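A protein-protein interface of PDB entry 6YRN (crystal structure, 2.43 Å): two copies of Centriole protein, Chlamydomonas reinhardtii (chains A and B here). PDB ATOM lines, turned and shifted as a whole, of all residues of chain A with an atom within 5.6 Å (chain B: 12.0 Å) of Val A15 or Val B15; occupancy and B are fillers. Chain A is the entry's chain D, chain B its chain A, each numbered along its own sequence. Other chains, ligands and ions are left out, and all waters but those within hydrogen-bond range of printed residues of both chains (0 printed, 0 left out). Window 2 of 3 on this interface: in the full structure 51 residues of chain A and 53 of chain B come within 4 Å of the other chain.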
ATOM      1  N   LEU A  11      14.457   0.573 -27.431  1.00  0.00           N
ATOM      2  CA  LEU A  11      15.098  -0.516 -26.693  1.00  0.00           C
ATOM      3  C   LEU A  11      16.246  -1.102 -27.513  1.00  0.00           C
ATOM      4  O   LEU A  11      17.292  -1.419 -26.950  1.00  0.00           O
ATOM      5  CB  LEU A  11      14.088  -1.631 -26.331  1.00  0.00           C
ATOM      6  CG  LEU A  11      12.981  -1.290 -25.319  1.00  0.00           C
ATOM      7  CD1 LEU A  11      11.910  -2.386 -25.279  1.00  0.00           C
ATOM      8  CD2 LEU A  11      13.556  -1.042 -23.914  1.00  0.00           C
ATOM      9  N   ASP A  12      16.043  -1.255 -28.838  1.00  0.00           N
ATOM     10  CA  ASP A  12      17.038  -1.768 -29.791  1.00  0.00           C
ATOM     11  C   ASP A  12      18.251  -0.864 -29.865  1.00  0.00           C
ATOM     12  O   ASP A  12      19.366  -1.372 -29.985  1.00  0.00           O
ATOM     13  CB  ASP A  12      16.440  -1.949 -31.203  1.00  0.00           C
ATOM     14  CG  ASP A  12      15.509  -3.132 -31.345  1.00  0.00           C
ATOM     15  OD1 ASP A  12      15.529  -4.017 -30.453  1.00  0.00           O
ATOM     16  OD2 ASP A  12      14.717  -3.150 -32.319  1.00  0.00           O
ATOM     17  N   THR A  13      18.029   0.473 -29.812  1.00  0.00           N
ATOM     18  CA  THR A  13      19.075   1.503 -29.838  1.00  0.00           C
ATOM     19  C   THR A  13      19.933   1.387 -28.581  1.00  0.00           C
ATOM     20  O   THR A  13      21.155   1.458 -28.671  1.00  0.00           O
ATOM     21  CB  THR A  13      18.493   2.936 -30.006  1.00  0.00           C
ATOM     22  OG1 THR A  13      17.588   3.231 -28.945  1.00  0.00           O
ATOM     23  CG2 THR A  13      17.847   3.179 -31.369  1.00  0.00           C
ATOM     24  N   LYS A  14      19.295   1.177 -27.421  1.00  0.00           N
ATOM     25  CA  LYS A  14      19.971   1.010 -26.135  1.00  0.00           C
ATOM     26  C   LYS A  14      20.928  -0.164 -26.189  1.00  0.00           C
ATOM     27  O   LYS A  14      22.113   0.035 -25.921  1.00  0.00           O
ATOM     28  CB  LYS A  14      18.977   0.840 -24.979  1.00  0.00           C
ATOM     29  CG  LYS A  14      18.230   2.107 -24.622  1.00  0.00           C
ATOM     30  CD  LYS A  14      17.368   1.870 -23.408  1.00  0.00           C
ATOM     31  CE  LYS A  14      16.360   2.962 -23.135  1.00  0.00           C
ATOM     32  NZ  LYS A  14      15.676   2.723 -21.832  1.00  0.00           N
ATOM     33  N   VAL A  15      20.438  -1.359 -26.608  1.00  0.00           N
ATOM     34  CA  VAL A  15      21.216  -2.597 -26.780  1.00  0.00           C
ATOM     35  C   VAL A  15      22.433  -2.310 -27.665  1.00  0.00           C
ATOM     36  O   VAL A  15      23.564  -2.592 -27.252  1.00  0.00           O
ATOM     37  CB  VAL A  15      20.353  -3.767 -27.338  1.00  0.00           C
ATOM     38  CG1 VAL A  15      21.216  -4.901 -27.889  1.00  0.00           C
ATOM     39  CG2 VAL A  15      19.394  -4.300 -26.281  1.00  0.00           C
ATOM     40  N   SER A  16      22.199  -1.703 -28.852  1.00  0.00           N
ATOM     41  CA  SER A  16      23.231  -1.322 -29.819  1.00  0.00           C
ATOM     42  C   SER A  16      24.266  -0.380 -29.197  1.00  0.00           C
ATOM     43  O   SER A  16      25.460  -0.664 -29.288  1.00  0.00           O
ATOM     44  CB  SER A  16      22.595  -0.686 -31.054  1.00  0.00           C
ATOM     45  OG  SER A  16      23.551  -0.323 -32.033  1.00  0.00           O
ATOM     46  N   GLU A  17      23.805   0.706 -28.535  1.00  0.00           N
ATOM     47  CA  GLU A  17      24.634   1.713 -27.867  1.00  0.00           C
ATOM     48  C   GLU A  17      25.532   1.075 -26.794  1.00  0.00           C
ATOM     49  O   GLU A  17      26.732   1.321 -26.784  1.00  0.00           O
ATOM     50  CB  GLU A  17      23.752   2.823 -27.260  1.00  0.00           C
ATOM     51  CG  GLU A  17      24.507   3.860 -26.449  1.00  0.00           C
ATOM     52  CD  GLU A  17      23.620   4.735 -25.590  1.00  0.00           C
ATOM     53  OE1 GLU A  17      23.369   4.363 -24.421  1.00  0.00           O
ATOM     54  OE2 GLU A  17      23.173   5.794 -26.088  1.00  0.00           O
ATOM     55  N   LEU A  18      24.950   0.247 -25.923  1.00  0.00           N
ATOM     56  CA  LEU A  18      25.638  -0.437 -24.840  1.00  0.00           C
ATOM     57  C   LEU A  18      26.596  -1.484 -25.353  1.00  0.00           C
ATOM     58  O   LEU A  18      27.672  -1.641 -24.767  1.00  0.00           O
ATOM     59  CB  LEU A  18      24.622  -1.059 -23.859  1.00  0.00           C
ATOM     60  CG  LEU A  18      23.847  -0.112 -22.934  1.00  0.00           C
ATOM     61  CD1 LEU A  18      22.650  -0.821 -22.324  1.00  0.00           C
ATOM     62  CD2 LEU A  18      24.722   0.416 -21.811  1.00  0.00           C
ATOM     63  N   SER A  19      26.229  -2.202 -26.430  1.00  0.00           N
ATOM     64  CA  SER A  19      27.096  -3.238 -27.009  1.00  0.00           C
ATOM     65  C   SER A  19      28.402  -2.645 -27.523  1.00  0.00           C
ATOM     66  O   SER A  19      29.467  -3.201 -27.249  1.00  0.00           O
ATOM     67  CB  SER A  19      26.390  -3.975 -28.137  1.00  0.00           C
ATOM     68  OG  SER A  19      25.474  -4.909 -27.596  1.00  0.00           O
ATOM     69  N   HIS A  20      28.303  -1.510 -28.261  1.00  0.00           N
ATOM     70  CA  HIS A  20      29.416  -0.750 -28.832  1.00  0.00           C
ATOM     71  C   HIS A  20      30.247  -0.119 -27.737  1.00  0.00           C
ATOM     72  O   HIS A  20      31.468  -0.095 -27.870  1.00  0.00           O
ATOM     73  CB  HIS A  20      28.917   0.323 -29.817  1.00  0.00           C
ATOM     74  CG  HIS A  20      28.475  -0.217 -31.141  1.00  0.00           C
ATOM     75  ND1 HIS A  20      27.171  -0.056 -31.590  1.00  0.00           N
ATOM     76  CD2 HIS A  20      29.182  -0.891 -32.079  1.00  0.00           C
ATOM     77  CE1 HIS A  20      27.125  -0.647 -32.774  1.00  0.00           C
ATOM     78  NE2 HIS A  20      28.311  -1.170 -33.108  1.00  0.00           N
ATOM     79  N   GLU B  10      13.415 -10.183 -21.970  1.00  0.00           N
ATOM     80  CA  GLU B  10      14.122 -10.561 -23.193  1.00  0.00           C
ATOM     81  C   GLU B  10      15.211  -9.545 -23.601  1.00  0.00           C
ATOM     82  O   GLU B  10      16.397  -9.829 -23.393  1.00  0.00           O
ATOM     83  CB  GLU B  10      13.127 -10.825 -24.339  1.00  0.00           C
ATOM     84  CG  GLU B  10      12.294 -12.087 -24.170  1.00  0.00           C
ATOM     85  CD  GLU B  10      11.363 -12.409 -25.325  1.00  0.00           C
ATOM     86  OE1 GLU B  10      11.413 -11.694 -26.354  1.00  0.00           O
ATOM     87  OE2 GLU B  10      10.589 -13.387 -25.207  1.00  0.00           O
ATOM     88  N   LEU B  11      14.804  -8.381 -24.207  1.00  0.00           N
ATOM     89  CA  LEU B  11      15.704  -7.293 -24.628  1.00  0.00           C
ATOM     90  C   LEU B  11      16.122  -6.461 -23.407  1.00  0.00           C
ATOM     91  O   LEU B  11      17.261  -5.996 -23.347  1.00  0.00           O
ATOM     92  CB  LEU B  11      15.066  -6.380 -25.704  1.00  0.00           C
ATOM     93  CG  LEU B  11      14.788  -6.974 -27.112  1.00  0.00           C
ATOM     94  CD1 LEU B  11      14.021  -5.988 -27.970  1.00  0.00           C
ATOM     95  CD2 LEU B  11      16.068  -7.364 -27.844  1.00  0.00           C
ATOM     96  N   ASP B  12      15.206  -6.308 -22.420  1.00  0.00           N
ATOM     97  CA  ASP B  12      15.454  -5.595 -21.161  1.00  0.00           C
ATOM     98  C   ASP B  12      16.515  -6.340 -20.312  1.00  0.00           C
ATOM     99  O   ASP B  12      17.316  -5.675 -19.652  1.00  0.00           O
ATOM    100  CB  ASP B  12      14.141  -5.377 -20.377  1.00  0.00           C
ATOM    101  CG  ASP B  12      13.168  -4.401 -21.019  1.00  0.00           C
ATOM    102  OD1 ASP B  12      13.626  -3.519 -21.792  1.00  0.00           O
ATOM    103  OD2 ASP B  12      11.948  -4.514 -20.749  1.00  0.00           O
ATOM    104  N   THR B  13      16.536  -7.713 -20.350  1.00  0.00           N
ATOM    105  CA  THR B  13      17.530  -8.562 -19.641  1.00  0.00           C
ATOM    106  C   THR B  13      18.921  -8.418 -20.299  1.00  0.00           C
ATOM    107  O   THR B  13      19.940  -8.469 -19.607  1.00  0.00           O
ATOM    108  CB  THR B  13      17.108 -10.058 -19.551  1.00  0.00           C
ATOM    109  OG1 THR B  13      17.212 -10.690 -20.831  1.00  0.00           O
ATOM    110  CG2 THR B  13      15.713 -10.264 -18.944  1.00  0.00           C
ATOM    111  N   LYS B  14      18.947  -8.251 -21.647  1.00  0.00           N
ATOM    112  CA  LYS B  14      20.162  -8.029 -22.445  1.00  0.00           C
ATOM    113  C   LYS B  14      20.733  -6.666 -22.059  1.00  0.00           C
ATOM    114  O   LYS B  14      21.935  -6.561 -21.845  1.00  0.00           O
ATOM    115  CB  LYS B  14      19.897  -8.084 -23.969  1.00  0.00           C
ATOM    116  CG  LYS B  14      19.614  -9.476 -24.528  1.00  0.00           C
ATOM    117  CD  LYS B  14      19.321  -9.423 -26.035  1.00  0.00           C
ATOM    118  CE  LYS B  14      18.776 -10.724 -26.572  1.00  0.00           C
ATOM    119  NZ  LYS B  14      18.633 -10.691 -28.049  1.00  0.00           N
ATOM    120  N   VAL B  15      19.855  -5.640 -21.916  1.00  0.00           N
ATOM    121  CA  VAL B  15      20.227  -4.284 -21.498  1.00  0.00           C
ATOM    122  C   VAL B  15      20.836  -4.337 -20.104  1.00  0.00           C
ATOM    123  O   VAL B  15      21.904  -3.768 -19.893  1.00  0.00           O
ATOM    124  CB  VAL B  15      19.061  -3.256 -21.619  1.00  0.00           C
ATOM    125  CG1 VAL B  15      19.357  -1.954 -20.875  1.00  0.00           C
ATOM    126  CG2 VAL B  15      18.750  -2.957 -23.078  1.00  0.00           C
ATOM    127  N   SER B  16      20.202  -5.064 -19.175  1.00  0.00           N
ATOM    128  CA  SER B  16      20.722  -5.218 -17.811  1.00  0.00           C
ATOM    129  C   SER B  16      22.079  -5.920 -17.848  1.00  0.00           C
ATOM    130  O   SER B  16      23.044  -5.401 -17.280  1.00  0.00           O
ATOM    131  CB  SER B  16      19.731  -5.960 -16.910  1.00  0.00           C
ATOM    132  OG  SER B  16      19.748  -7.366 -17.108  1.00  0.00           O
ATOM    133  N   GLU B  17      22.166  -7.041 -18.601  1.00  0.00           N
ATOM    134  CA  GLU B  17      23.400  -7.815 -18.791  1.00  0.00           C
ATOM    135  C   GLU B  17      24.569  -6.938 -19.302  1.00  0.00           C
ATOM    136  O   GLU B  17      25.647  -6.974 -18.713  1.00  0.00           O
ATOM    137  CB  GLU B  17      23.148  -9.041 -19.706  1.00  0.00           C
ATOM    138  CG  GLU B  17      24.209 -10.141 -19.634  1.00  0.00           C
ATOM    139  CD  GLU B  17      24.350 -10.984 -18.375  1.00  0.00           C
ATOM    140  OE1 GLU B  17      25.407 -11.641 -18.233  1.00  0.00           O
ATOM    141  OE2 GLU B  17      23.411 -11.008 -17.544  1.00  0.00           O
ATOM    142  N   LEU B  18      24.326  -6.116 -20.333  1.00  0.00           N
ATOM    143  CA  LEU B  18      25.300  -5.211 -20.932  1.00  0.00           C
ATOM    144  C   LEU B  18      25.767  -4.129 -19.984  1.00  0.00           C
ATOM    145  O   LEU B  18      26.960  -3.864 -19.958  1.00  0.00           O
ATOM    146  CB  LEU B  18      24.751  -4.536 -22.200  1.00  0.00           C
ATOM    147  CG  LEU B  18      24.398  -5.404 -23.387  1.00  0.00           C
ATOM    148  CD1 LEU B  18      23.609  -4.604 -24.412  1.00  0.00           C
ATOM    149  CD2 LEU B  18      25.627  -6.024 -24.014  1.00  0.00           C
ATOM    150  N   SER B  19      24.844  -3.462 -19.255  1.00  0.00           N
ATOM    151  CA  SER B  19      25.153  -2.360 -18.320  1.00  0.00           C
ATOM    152  C   SER B  19      26.087  -2.850 -17.185  1.00  0.00           C
ATOM    153  O   SER B  19      27.075  -2.182 -16.869  1.00  0.00           O
ATOM    154  CB  SER B  19      23.866  -1.763 -17.739  1.00  0.00           C
ATOM    155  OG  SER B  19      23.114  -1.014 -18.680  1.00  0.00           O
ATOM    156  N   HIS B  20      25.774  -4.030 -16.615  1.00  0.00           N
ATOM    157  CA  HIS B  20      26.553  -4.701 -15.587  1.00  0.00           C
ATOM    158  C   HIS B  20      27.982  -5.018 -16.119  1.00  0.00           C
ATOM    159  O   HIS B  20      28.969  -4.701 -15.455  1.00  0.00           O
ATOM    160  CB  HIS B  20      25.831  -5.985 -15.131  1.00  0.00           C
ATOM    161  CG  HIS B  20      26.519  -6.685 -13.988  1.00  0.00           C
ATOM    162  ND1 HIS B  20      27.633  -7.485 -14.198  1.00  0.00           N
ATOM    163  CD2 HIS B  20      26.254  -6.653 -12.660  1.00  0.00           C
ATOM    164  CE1 HIS B  20      28.014  -7.895 -13.003  1.00  0.00           C
ATOM    165  NE2 HIS B  20      27.221  -7.420 -12.046  1.00  0.00           N
ATOM    166  N   LYS B  21      28.065  -5.588 -17.350  1.00  0.00           N
ATOM    167  CA  LYS B  21      29.310  -5.942 -18.032  1.00  0.00           C
ATOM    168  C   LYS B  21      30.123  -4.700 -18.343  1.00  0.00           C
ATOM    169  O   LYS B  21      31.352  -4.748 -18.260  1.00  0.00           O
ATOM    170  CB  LYS B  21      29.033  -6.759 -19.302  1.00  0.00           C
ATOM    171  CG  LYS B  21      28.755  -8.241 -19.024  1.00  0.00           C
ATOM    172  CD  LYS B  21      28.493  -8.987 -20.317  1.00  0.00           C
ATOM    173  CE  LYS B  21      27.951 -10.373 -20.098  1.00  0.00           C
ATOM    174  NZ  LYS B  21      27.195 -10.857 -21.286  1.00  0.00           N
ATOM    175  N   LEU B  22      29.438  -3.584 -18.662  1.00  0.00           N
ATOM    176  CA  LEU B  22      30.072  -2.303 -18.968  1.00  0.00           C
ATOM    177  C   LEU B  22      30.729  -1.710 -17.712  1.00  0.00           C
ATOM    178  O   LEU B  22      31.885  -1.307 -17.767  1.00  0.00           O
ATOM    179  CB  LEU B  22      29.078  -1.316 -19.632  1.00  0.00           C
ATOM    180  CG  LEU B  22      29.613   0.090 -19.966  1.00  0.00           C
ATOM    181  CD1 LEU B  22      30.694   0.038 -21.027  1.00  0.00           C
ATOM    182  CD2 LEU B  22      28.501   1.038 -20.312  1.00  0.00           C
ATOM    183  N   GLY B  23      29.992  -1.692 -16.606  1.00  0.00           N
ATOM    184  CA  GLY B  23      30.484  -1.214 -15.320  1.00  0.00           C
ATOM    185  C   GLY B  23      31.722  -1.962 -14.855  1.00  0.00           C
ATOM    186  O   GLY B  23      32.679  -1.332 -14.401  1.00  0.00           O
ATOM    187  N   SER B  24      31.722  -3.317 -15.010  1.00  0.00           N
ATOM    188  CA  SER B  24      32.840  -4.207 -14.660  1.00  0.00           C
ATOM    189  C   SER B  24      34.070  -3.894 -15.510  1.00  0.00           C
ATOM    190  O   SER B  24      35.174  -3.809 -14.977  1.00  0.00           O
ATOM    191  CB  SER B  24      32.438  -5.672 -14.819  1.00  0.00           C
ATOM    192  OG  SER B  24      31.617  -6.131 -13.757  1.00  0.00           O
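O of Val B15 is in hydrogen-bond range of OG of Ser B19 (3.2 Å). The backbone carbonyl oxygen (O) of Val A15 lies within hydrogen-bond range of the side-chain hydroxyl (OG) of Ser A19.
Among the printed residues, merely in contact across the chains: Leu A11 with Asp B12, Val A15 with Leu B18, Asp A12 with Leu B11, Val A15 with Val B15, Leu A18 with Ser B19, Ser A19 with Leu B18, Leu A18 with Leu B18 and Leu A18 with Val B15.
Of the printed residues of chain B, Asp A12 touches Leu B11 (3.5 Å). No residue of chain B comes within 4 Å of Lys A14. Of the printed residues of chain B, Val A15 touches Val B15 and Leu B18. No residue of chain B comes within 4 Å of Ser A16. No residue of chain B comes within 4 Å of Glu A17. Ser A19 touches just one residue of chain B: Leu B18. Lys B14 touches none of the printed residues of chain A. Of chain A, only Val A15 (3.5 Å) and Leu A18 (3.8 Å) come within 4 Å of Val B15. Glu B17 touches none of the printed residues of chain A. Printed residues of chain A within 4 Å of Leu B18: Val A15, Leu A18 and Ser A19. Printed residues of chain A within 4 Å of Ser B19: Leu A18 (3.7 Å). The nearest printed residue of chain B that does not touch Val A15 is Leu B11 (4.004 Å).
Of the 15 printed residues of chain B, 5 touch a printed residue of chain A. Printed residues of chain B that touch a printed residue of chain A: Leu B11, Asp B12, Val B15, Leu B18 and Ser B19. Hydrophobic or aromatic side chains of chain B that line the printed part of chain A: Leu B11, Val B15 and Leu B18. Printed residues of chain A that touch a printed residue of chain B: Leu A11, Asp A12, Val A15, Leu A18 and Ser A19. Among the printed residues, no Asp or Glu carboxylate lies within 4 Å of a Lys or Arg side-chain nitrogen of the other chain.
Leu A11 touches Asp B12, and with the chains exchanged Asp A12 touches Leu B11. Val A15 touches its own counterpart, Val B15. Val A15 touches Leu B18, and with the chains exchanged Leu A18 touches Val B15. Leu A18 touches its own counterpart, Leu B18. 10 positions are printed for both chains.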
